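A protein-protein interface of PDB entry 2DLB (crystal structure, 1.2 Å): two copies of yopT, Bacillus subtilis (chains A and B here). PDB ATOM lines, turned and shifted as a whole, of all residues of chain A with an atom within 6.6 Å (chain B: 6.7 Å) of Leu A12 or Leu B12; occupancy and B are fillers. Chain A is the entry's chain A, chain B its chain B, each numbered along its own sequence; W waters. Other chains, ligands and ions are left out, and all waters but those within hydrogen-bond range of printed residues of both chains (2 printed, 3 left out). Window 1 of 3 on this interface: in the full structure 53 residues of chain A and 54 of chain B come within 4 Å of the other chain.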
ATOM      1  N   ILE A   8      22.160  -0.098  -8.245  1.00  0.00           N
ATOM      2  CA  ILE A   8      22.692   1.209  -8.552  1.00  0.00           C
ATOM      3  C   ILE A   8      23.669   1.603  -7.437  1.00  0.00           C
ATOM      4  O   ILE A   8      23.353   1.514  -6.259  1.00  0.00           O
ATOM      5  CB  ILE A   8      21.579   2.249  -8.718  1.00  0.00           C
ATOM      6  CG1 ILE A   8      20.450   1.791  -9.685  1.00  0.00           C
ATOM      7  CG2 ILE A   8      22.141   3.558  -9.162  1.00  0.00           C
ATOM      8  CD1 ILE A   8      19.255   1.151  -8.955  1.00  0.00           C
ATOM      9  N   ALA A   9      24.836   2.068  -7.827  1.00  0.00           N
ATOM     10  CA  ALA A   9      25.846   2.643  -6.957  1.00  0.00           C
ATOM     11  C   ALA A   9      25.577   4.142  -6.849  1.00  0.00           C
ATOM     12  O   ALA A   9      25.571   4.853  -7.849  1.00  0.00           O
ATOM     13  CB  ALA A   9      27.239   2.392  -7.495  1.00  0.00           C
ATOM     14  N   LEU A  10      25.370   4.603  -5.609  1.00  0.00           N
ATOM     15  CA  LEU A  10      25.251   6.016  -5.315  1.00  0.00           C
ATOM     16  C   LEU A  10      26.482   6.473  -4.533  1.00  0.00           C
ATOM     17  O   LEU A  10      26.780   5.888  -3.479  1.00  0.00           O
ATOM     18  CB  LEU A  10      24.026   6.328  -4.469  1.00  0.00           C
ATOM     19  CG  LEU A  10      22.714   5.685  -4.876  1.00  0.00           C
ATOM     20  CD1 LEU A  10      21.602   6.175  -3.947  1.00  0.00           C
ATOM     21  CD2 LEU A  10      22.383   5.943  -6.316  1.00  0.00           C
ATOM     22  N   ASN A  11      27.159   7.473  -5.049  1.00  0.00           N
ATOM     23  CA  ASN A  11      28.295   8.059  -4.353  1.00  0.00           C
ATOM     24  C   ASN A  11      27.893   9.417  -3.854  1.00  0.00           C
ATOM     25  O   ASN A  11      27.715  10.351  -4.611  1.00  0.00           O
ATOM     26  CB  ASN A  11      29.469   8.163  -5.332  1.00  0.00           C
ATOM     27  CG  ASN A  11      29.767   6.814  -5.984  1.00  0.00           C
ATOM     28  OD1 ASN A  11      29.789   6.714  -7.208  1.00  0.00           O
ATOM     29  ND2 ASN A  11      29.981   5.826  -5.129  1.00  0.00           N
ATOM     30  N   LEU A  12      27.703   9.492  -2.557  1.00  0.00           N
ATOM     31  CA  LEU A  12      27.248  10.667  -1.881  1.00  0.00           C
ATOM     32  C   LEU A  12      28.394  11.322  -1.106  1.00  0.00           C
ATOM     33  O   LEU A  12      29.285  10.652  -0.641  1.00  0.00           O
ATOM     34  CB  LEU A  12      26.185  10.320  -0.838  1.00  0.00           C
ATOM     35  CG  LEU A  12      25.038   9.425  -1.332  1.00  0.00           C
ATOM     36  CD1 LEU A  12      24.008   9.281  -0.211  1.00  0.00           C
ATOM     37  CD2 LEU A  12      24.413   9.921  -2.594  1.00  0.00           C
ATOM     38  N   GLU A  13      28.325  12.633  -0.936  1.00  0.00           N
ATOM     39  CA  GLU A  13      29.155  13.349  -0.004  1.00  0.00           C
ATOM     40  C   GLU A  13      28.221  14.085   0.964  1.00  0.00           C
ATOM     41  O   GLU A  13      27.316  14.805   0.546  1.00  0.00           O
ATOM     42  CB  GLU A  13      30.102  14.336  -0.708  1.00  0.00           C
ATOM     43  CG  GLU A  13      31.232  14.753   0.220  1.00  0.00           C
ATOM     44  CD  GLU A  13      32.332  13.721   0.345  1.00  0.00           C
ATOM     45  OE1 GLU A  13      32.434  12.737  -0.407  1.00  0.00           O
ATOM     46  OE2 GLU A  13      33.161  13.906   1.281  1.00  0.00           O
ATOM     47  N   ILE A  14      28.418  13.890   2.245  1.00  0.00           N
ATOM     48  CA  ILE A  14      27.628  14.507   3.315  1.00  0.00           C
ATOM     49  C   ILE A  14      28.550  15.379   4.167  1.00  0.00           C
ATOM     50  O   ILE A  14      29.789  15.269   4.127  1.00  0.00           O
ATOM     51  CB  ILE A  14      26.892  13.507   4.198  1.00  0.00           C
ATOM     52  CG1 ILE A  14      27.814  12.564   4.946  1.00  0.00           C
ATOM     53  CG2 ILE A  14      25.888  12.702   3.342  1.00  0.00           C
ATOM     54  CD1 ILE A  14      27.241  12.028   6.247  1.00  0.00           C
ATOM     55  N   VAL A  43      17.300   3.656   2.782  1.00  0.00           N
ATOM     56  CA  VAL A  43      17.779   5.024   2.679  1.00  0.00           C
ATOM     57  C   VAL A  43      16.686   5.867   2.030  1.00  0.00           C
ATOM     58  O   VAL A  43      15.959   5.420   1.161  1.00  0.00           O
ATOM     59  CB  VAL A  43      19.102   5.086   1.890  1.00  0.00           C
ATOM     60  CG1 VAL A  43      18.971   4.584   0.453  1.00  0.00           C
ATOM     61  CG2 VAL A  43      19.710   6.495   1.942  1.00  0.00           C
ATOM     62  N   PHE A  45      15.764   9.921   0.465  1.00  0.00           N
ATOM     63  CA  PHE A  45      16.248  11.200  -0.046  1.00  0.00           C
ATOM     64  C   PHE A  45      15.141  12.247   0.055  1.00  0.00           C
ATOM     65  O   PHE A  45      14.025  11.996  -0.383  1.00  0.00           O
ATOM     66  CB  PHE A  45      16.701  11.100  -1.495  1.00  0.00           C
ATOM     67  CG  PHE A  45      17.972  10.291  -1.628  1.00  0.00           C
ATOM     68  CD1 PHE A  45      17.943   8.945  -1.678  1.00  0.00           C
ATOM     69  CD2 PHE A  45      19.184  10.960  -1.642  1.00  0.00           C
ATOM     70  CE1 PHE A  45      19.115   8.219  -1.739  1.00  0.00           C
ATOM     71  CE2 PHE A  45      20.345  10.226  -1.725  1.00  0.00           C
ATOM     72  CZ  PHE A  45      20.330   8.864  -1.771  1.00  0.00           C
ATOM     73  N   LEU A  57      18.321  -0.442   0.580  1.00  0.00           N
ATOM     74  CA  LEU A  57      19.767  -0.307   0.647  1.00  0.00           C
ATOM     75  C   LEU A  57      20.393  -1.670   0.852  1.00  0.00           C
ATOM     76  O   LEU A  57      20.063  -2.324   1.864  1.00  0.00           O
ATOM     77  CB  LEU A  57      20.119   0.622   1.810  1.00  0.00           C
ATOM     78  CG  LEU A  57      21.548   0.985   2.040  1.00  0.00           C
ATOM     79  CD1 LEU A  57      22.141   1.689   0.816  1.00  0.00           C
ATOM     80  CD2 LEU A  57      21.653   1.868   3.281  1.00  0.00           C
ATOM     81  N   SER A  58      21.227  -2.082  -0.093  1.00  0.00           N
ATOM     82  CA  SER A  58      21.910  -3.354  -0.184  1.00  0.00           C
ATOM     83  C   SER A  58      23.290  -3.386   0.460  1.00  0.00           C
ATOM     84  O   SER A  58      23.750  -4.445   0.923  1.00  0.00           O
ATOM     85  CB  SER A  58      22.078  -3.751  -1.672  1.00  0.00           C
ATOM     86  OG  SER A  58      22.445  -2.640  -2.471  1.00  0.00           O
ATOM     87  N   ASP A  59      23.976  -2.264   0.449  1.00  0.00           N
ATOM     88  CA  ASP A  59      25.356  -2.158   0.895  1.00  0.00           C
ATOM     89  C   ASP A  59      25.702  -0.756   1.205  1.00  0.00           C
ATOM     90  O   ASP A  59      25.156   0.117   0.554  1.00  0.00           O
ATOM     91  CB  ASP A  59      26.359  -2.651  -0.211  1.00  0.00           C
ATOM     92  CG  ASP A  59      27.782  -2.682   0.294  1.00  0.00           C
ATOM     93  OD1 ASP A  59      27.952  -3.231   1.405  1.00  0.00           O
ATOM     94  OD2 ASP A  59      28.732  -2.185  -0.346  1.00  0.00           O
ATOM     95  N   MET A  60      26.606  -0.555   2.146  1.00  0.00           N
ATOM     96  CA  MET A  60      27.158   0.747   2.429  1.00  0.00           C
ATOM     97  C   MET A  60      28.627   0.666   2.814  1.00  0.00           C
ATOM     98  O   MET A  60      28.947  -0.239   3.576  1.00  0.00           O
ATOM     99  CB  MET A  60      26.460   1.402   3.643  1.00  0.00           C
ATOM    100  CG  MET A  60      27.154   2.746   3.946  1.00  0.00           C
ATOM    101  SD  MET A  60      26.319   3.308   5.512  1.00  0.00           S
ATOM    102  CE  MET A  60      27.499   4.781   5.793  1.00  0.00           C
ATOM    103  N   GLU A  61      29.385   1.617   2.319  1.00  0.00           N
ATOM    104  CA  GLU A  61      30.752   1.820   2.778  1.00  0.00           C
ATOM    105  C   GLU A  61      30.904   3.317   2.992  1.00  0.00           C
ATOM    106  O   GLU A  61      30.145   4.079   2.403  1.00  0.00           O
ATOM    107  CB  GLU A  61      31.778   1.273   1.819  1.00  0.00           C
ATOM    108  CG  GLU A  61      31.784  -0.249   1.656  1.00  0.00           C
ATOM    109  CD  GLU A  61      31.065  -0.505   0.332  1.00  0.00           C
ATOM    110  OE1 GLU A  61      30.939  -1.697   0.008  1.00  0.00           O
ATOM    111  OE2 GLU A  61      30.688   0.506  -0.326  1.00  0.00           O
ATOM    112  N   ILE B   8      32.132  13.527   4.434  1.00  0.00           N
ATOM    113  CA  ILE B   8      32.216  12.073   4.420  1.00  0.00           C
ATOM    114  C   ILE B   8      31.653  11.554   3.125  1.00  0.00           C
ATOM    115  O   ILE B   8      30.570  12.004   2.678  1.00  0.00           O
ATOM    116  CB  ILE B   8      31.436  11.470   5.616  1.00  0.00           C
ATOM    117  CG1 ILE B   8      31.862  12.099   6.963  1.00  0.00           C
ATOM    118  CG2 ILE B   8      31.606   9.978   5.641  1.00  0.00           C
ATOM    119  CD1 ILE B   8      30.860  12.987   7.579  1.00  0.00           C
ATOM    120  N   ALA B   9      32.379  10.660   2.486  1.00  0.00           N
ATOM    121  CA  ALA B   9      31.932   9.946   1.306  1.00  0.00           C
ATOM    122  C   ALA B   9      31.155   8.718   1.709  1.00  0.00           C
ATOM    123  O   ALA B   9      31.708   7.903   2.437  1.00  0.00           O
ATOM    124  CB  ALA B   9      33.134   9.564   0.437  1.00  0.00           C
ATOM    125  N   LEU B  10      29.929   8.602   1.253  1.00  0.00           N
ATOM    126  CA  LEU B  10      29.123   7.400   1.449  1.00  0.00           C
ATOM    127  C   LEU B  10      28.942   6.709   0.109  1.00  0.00           C
ATOM    128  O   LEU B  10      28.463   7.334  -0.820  1.00  0.00           O
ATOM    129  CB  LEU B  10      27.766   7.727   2.058  1.00  0.00           C
ATOM    130  CG  LEU B  10      27.669   8.671   3.238  1.00  0.00           C
ATOM    131  CD1 LEU B  10      26.191   8.869   3.668  1.00  0.00           C
ATOM    132  CD2 LEU B  10      28.465   8.218   4.450  1.00  0.00           C
ATOM    133  N   ASN B  11      29.303   5.471   0.024  1.00  0.00           N
ATOM    134  CA  ASN B  11      29.140   4.665  -1.170  1.00  0.00           C
ATOM    135  C   ASN B  11      28.051   3.631  -0.909  1.00  0.00           C
ATOM    136  O   ASN B  11      28.252   2.703  -0.134  1.00  0.00           O
ATOM    137  CB  ASN B  11      30.474   4.025  -1.503  1.00  0.00           C
ATOM    138  CG  ASN B  11      31.478   5.162  -1.691  1.00  0.00           C
ATOM    139  OD1 ASN B  11      31.253   6.051  -2.533  1.00  0.00           O
ATOM    140  ND2 ASN B  11      32.533   5.123  -0.898  1.00  0.00           N
ATOM    141  N   LEU B  12      26.899   3.864  -1.513  1.00  0.00           N
ATOM    142  CA  LEU B  12      25.716   3.078  -1.290  1.00  0.00           C
ATOM    143  C   LEU B  12      25.401   2.202  -2.506  1.00  0.00           C
ATOM    144  O   LEU B  12      25.683   2.631  -3.637  1.00  0.00           O
ATOM    145  CB  LEU B  12      24.497   3.963  -1.076  1.00  0.00           C
ATOM    146  CG  LEU B  12      24.598   5.019   0.034  1.00  0.00           C
ATOM    147  CD1 LEU B  12      23.238   5.659   0.217  1.00  0.00           C
ATOM    148  CD2 LEU B  12      25.141   4.440   1.346  1.00  0.00           C
ATOM    149  N   GLU B  13      24.789   1.057  -2.288  1.00  0.00           N
ATOM    150  CA  GLU B  13      24.229   0.260  -3.355  1.00  0.00           C
ATOM    151  C   GLU B  13      22.722   0.108  -3.025  1.00  0.00           C
ATOM    152  O   GLU B  13      22.376  -0.402  -1.954  1.00  0.00           O
ATOM    153  CB  GLU B  13      24.885  -1.091  -3.531  1.00  0.00           C
ATOM    154  CG  GLU B  13      24.634  -1.742  -4.885  1.00  0.00           C
ATOM    155  CD  GLU B  13      25.419  -1.143  -6.039  1.00  0.00           C
ATOM    156  OE1 GLU B  13      26.412  -0.393  -5.839  1.00  0.00           O
ATOM    157  OE2 GLU B  13      25.057  -1.397  -7.232  1.00  0.00           O
ATOM    158  N   ILE B  14      21.897   0.598  -3.969  1.00  0.00           N
ATOM    159  CA  ILE B  14      20.465   0.491  -3.811  1.00  0.00           C
ATOM    160  C   ILE B  14      19.865  -0.436  -4.869  1.00  0.00           C
ATOM    161  O   ILE B  14      20.521  -0.741  -5.873  1.00  0.00           O
ATOM    162  CB  ILE B  14      19.728   1.864  -3.857  1.00  0.00           C
ATOM    163  CG1 ILE B  14      19.928   2.566  -5.203  1.00  0.00           C
ATOM    164  CG2 ILE B  14      20.133   2.720  -2.660  1.00  0.00           C
ATOM    165  CD1 ILE B  14      18.897   3.665  -5.462  1.00  0.00           C
ATOM    166  N   VAL B  43      19.882  13.208   3.087  1.00  0.00           N
ATOM    167  CA  VAL B  43      19.794  11.748   2.988  1.00  0.00           C
ATOM    168  C   VAL B  43      19.599  11.196   4.374  1.00  0.00           C
ATOM    169  O   VAL B  43      20.206  11.696   5.349  1.00  0.00           O
ATOM    170  CB  VAL B  43      21.031  11.133   2.301  1.00  0.00           C
ATOM    171  CG1 VAL B  43      22.300  11.424   3.053  1.00  0.00           C
ATOM    172  CG2 VAL B  43      20.890   9.639   2.045  1.00  0.00           C
ATOM    173  N   PHE B  45      18.840   7.571   6.922  1.00  0.00           N
ATOM    174  CA  PHE B  45      19.004   6.119   7.066  1.00  0.00           C
ATOM    175  C   PHE B  45      18.122   5.613   8.192  1.00  0.00           C
ATOM    176  O   PHE B  45      18.126   6.184   9.292  1.00  0.00           O
ATOM    177  CB  PHE B  45      20.452   5.756   7.352  1.00  0.00           C
ATOM    178  CG  PHE B  45      21.378   6.126   6.215  1.00  0.00           C
ATOM    179  CD1 PHE B  45      21.972   7.383   6.123  1.00  0.00           C
ATOM    180  CD2 PHE B  45      21.657   5.209   5.230  1.00  0.00           C
ATOM    181  CE1 PHE B  45      22.804   7.720   5.061  1.00  0.00           C
ATOM    182  CE2 PHE B  45      22.469   5.525   4.133  1.00  0.00           C
ATOM    183  CZ  PHE B  45      23.033   6.793   4.086  1.00  0.00           C
ATOM    184  N   LEU B  57      23.313  16.677   2.530  1.00  0.00           N
ATOM    185  CA  LEU B  57      23.992  16.202   1.335  1.00  0.00           C
ATOM    186  C   LEU B  57      24.679  17.369   0.635  1.00  0.00           C
ATOM    187  O   LEU B  57      24.036  18.380   0.422  1.00  0.00           O
ATOM    188  CB  LEU B  57      22.951  15.579   0.462  1.00  0.00           C
ATOM    189  CG  LEU B  57      23.137  14.562  -0.580  1.00  0.00           C
ATOM    190  CD1 LEU B  57      24.117  13.470  -0.219  1.00  0.00           C
ATOM    191  CD2 LEU B  57      21.707  14.080  -0.836  1.00  0.00           C
ATOM    192  N   SER B  58      25.938  17.179   0.277  1.00  0.00           N
ATOM    193  CA  SER B  58      26.878  18.071  -0.372  1.00  0.00           C
ATOM    194  C   SER B  58      27.252  17.701  -1.816  1.00  0.00           C
ATOM    195  O   SER B  58      27.886  18.530  -2.504  1.00  0.00           O
ATOM    196  N   ASP B  59      26.912  16.521  -2.296  1.00  0.00           N
ATOM    197  CA  ASP B  59      27.161  16.070  -3.652  1.00  0.00           C
ATOM    198  C   ASP B  59      26.590  14.693  -3.852  1.00  0.00           C
ATOM    199  O   ASP B  59      26.525  13.948  -2.896  1.00  0.00           O
ATOM    200  CB  ASP B  59      28.668  15.985  -4.007  1.00  0.00           C
ATOM    201  CG  ASP B  59      28.952  15.809  -5.469  1.00  0.00           C
ATOM    202  OD1 ASP B  59      28.264  16.425  -6.307  1.00  0.00           O
ATOM    203  OD2 ASP B  59      29.859  15.032  -5.821  1.00  0.00           O
ATOM    204  N   MET B  60      26.255  14.379  -5.080  1.00  0.00           N
ATOM    205  CA  MET B  60      25.893  13.040  -5.451  1.00  0.00           C
ATOM    206  C   MET B  60      26.250  12.705  -6.888  1.00  0.00           C
ATOM    207  O   MET B  60      26.101  13.560  -7.747  1.00  0.00           O
ATOM    208  CB  MET B  60      24.373  12.945  -5.271  1.00  0.00           C
ATOM    209  CG  MET B  60      23.768  11.680  -5.753  1.00  0.00           C
ATOM    210  SD  MET B  60      21.944  11.616  -5.401  1.00  0.00           S
ATOM    211  CE  MET B  60      21.686  13.196  -4.338  1.00  0.00           C
ATOM    212  N   GLU B  61      26.651  11.476  -7.102  1.00  0.00           N
ATOM    213  CA  GLU B  61      26.805  10.894  -8.425  1.00  0.00           C
ATOM    214  C   GLU B  61      26.213   9.492  -8.364  1.00  0.00           C
ATOM    215  O   GLU B  61      26.090   8.900  -7.242  1.00  0.00           O
ATOM    216  CB  GLU B  61      28.282  10.809  -8.800  1.00  0.00           C
ATOM    217  CG  GLU B  61      29.074  12.090  -9.058  1.00  0.00           C
ATOM    218  CD  GLU B  61      30.437  11.729  -9.656  1.00  0.00           C
ATOM    219  OE1 GLU B  61      30.994  12.528 -10.413  1.00  0.00           O
ATOM    220  OE2 GLU B  61      30.896  10.602  -9.346  1.00  0.00           O
HETATM  221  O   HOH W   1      28.738   3.302  -4.307  1.00  0.00           O
HETATM  222  O   HOH W   2      29.703  12.341  -4.708  1.00  0.00           O
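Of chain B, only Ile B8 (3.8 Å), Ala B9 (3.4 Å), Leu B10 (2.9 Å), Leu B12 (3.7 Å), Val B43 (3.9 Å), Leu B57 (3.8 Å), Asp B59 (3.5 Å) and Met B60 (3.7 Å) come within 4 Å of Leu A12.
Printed residues of chain A within 4 Å of Leu B12: Ile A8, Ala A9, Leu A10, Leu A12, Leu A57, Asp A59 and Met A60.
Of the printed residues of chain A, Ile B8 touches Leu A12 (3.8 Å), Glu A13 (3.3 Å) and Ile A14 (2.9 Å).
Printed residues of chain B within 4 Å of Leu A10: Leu B10, Asn B11, Leu B12, Ile B14 and Glu B61.
Of the printed residues of chain A, Asn B11 touches Leu A10, Asn A11, Met A60 and Glu A61.
Of the printed residues of chain A, Ile B14 touches Ile A8 (2.9 Å), Leu A10 (3.97 Å), Val A43 (3.8 Å) and Ser A58 (3.6 Å).
The nearest residue of chain B that does not touch Leu A12 is Asn B11 (4.9 Å).
The nearest printed residue of chain A that does not touch Asn B11 is Asp A59 (4.1 Å).
Of the 14 printed residues of chain B, 14 touch a printed residue of chain A.
Hydrophobic or aromatic side chains of chain B within 4 Å of the printed part of chain A: Ile B8, Ala B9, Leu B10, Leu B12, Ile B14, Val B43, Phe B45, Leu B57 and Met B60.
Hydrophobic or aromatic side chains of chain A that line the printed part of chain B: Ile A8, Ala A9, Leu A10, Leu A12, Ile A14, Val A43, Phe A45, Leu A57 and Met A60.
Along chain A the printed residues that touch a printed residue of chain B span positions 8 to 61.
Among the printed residues, 46 pairs touch across the chains.
Among the printed residues, no Asp or Glu carboxylate lies within 4 Å of a Lys or Arg side-chain nitrogen of the other chain.
Ile A8 touches Glu B13, and with the chains exchanged Glu A13 touches Ile B8.
Asn A11 touches Met B60, and with the chains exchanged Met A60 touches Asn B11.
Leu B12 touches its own counterpart, Leu A12.
Val A43 touches its own counterpart, Val B43.
14 positions are printed for both chains.
Of the 46 pairs that touch across the chains among the printed residues, 42 have their exchanged pair printed and touching as well.
Leu A10 touches Ile B14 (CD1 to CG2, 3.97 Å).
Asn A11 touches Leu B10.
CA of Met B60 touches O of Asn A11, 3.4 Å away.
Ala B9 touches Glu A13 (CA to OE1, 3.3 Å).
Ile A14 touches Val B43 (CG2 to CG1, 3.8 Å).
Val A43 touches Val B43 (CG2 to CG2, 3.4 Å).
Leu A57 touches Leu B12 (CD1 to CB, 3.8 Å).
Asp A59 touches Leu B12.
Met A60 touches Asn B11 (CA to O, 3.4 Å).
Leu B12 touches Met A60 (CD2 to CG, 3.7 Å).
OE2 of Glu B13 sits close to N of Ile A8, at 3.3 Å.
O of Ile A8 sits at hydrogen-bond distance from N of Ile B14 (2.9 Å).
The backbone NH (N) of Leu A10 is in hydrogen-bond range of the backbone carbonyl oxygen (O) of Leu B12 (2.8 Å).
The side-chain amide oxygen of Asn B11 is in hydrogen-bond range of the side-chain amide nitrogen of Asn A11, 2.9 Å away.
The backbone carbonyl oxygen of Glu B61 is in hydrogen-bond range of the backbone NH of Asn A11.
The backbone carbonyl oxygen (O) of Leu A12 is in hydrogen-bond range of the backbone NH (N) of Leu B10.
The side-chain carboxylate (OE2) of Glu A13 lies within hydrogen-bond range of the backbone NH (N) of Ile B8 (3.3 Å).
O of Glu A13 is in hydrogen-bond range of N of Ser B58.
O of Asp B59 is in hydrogen-bond range of N of Glu A13.
The backbone NH (N) of Ile A14 sits at hydrogen-bond distance from the backbone carbonyl oxygen (O) of Ile B8.
The backbone NH (N) of Ser A58 lies within hydrogen-bond range of the backbone carbonyl oxygen (O) of Glu B13, at 2.8 Å.
The backbone NH (N) of Glu B13 lies within hydrogen-bond range of the backbone carbonyl oxygen (O) of Asp A59.
The backbone NH (N) of Asn B11 lies within hydrogen-bond range of the backbone carbonyl oxygen (O) of Glu A61, 2.9 Å away.
The backbone carbonyl oxygen (O) of Leu B10 lies close to the backbone carbonyl oxygen (O) of Leu A10, at 3.5 Å.
Water W2 bridges O of Asn A11 (2.8 Å) and OD2 of Asp B59 (2.9 Å).
Water W1 lies within hydrogen-bond range of the side-chain amide nitrogen (ND2) of Asn A11 (2.9 Å), the backbone carbonyl oxygen (O) of Leu B12 (3.2 Å) and the backbone carbonyl oxygen (O) of Leu A10 (3.3 Å).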
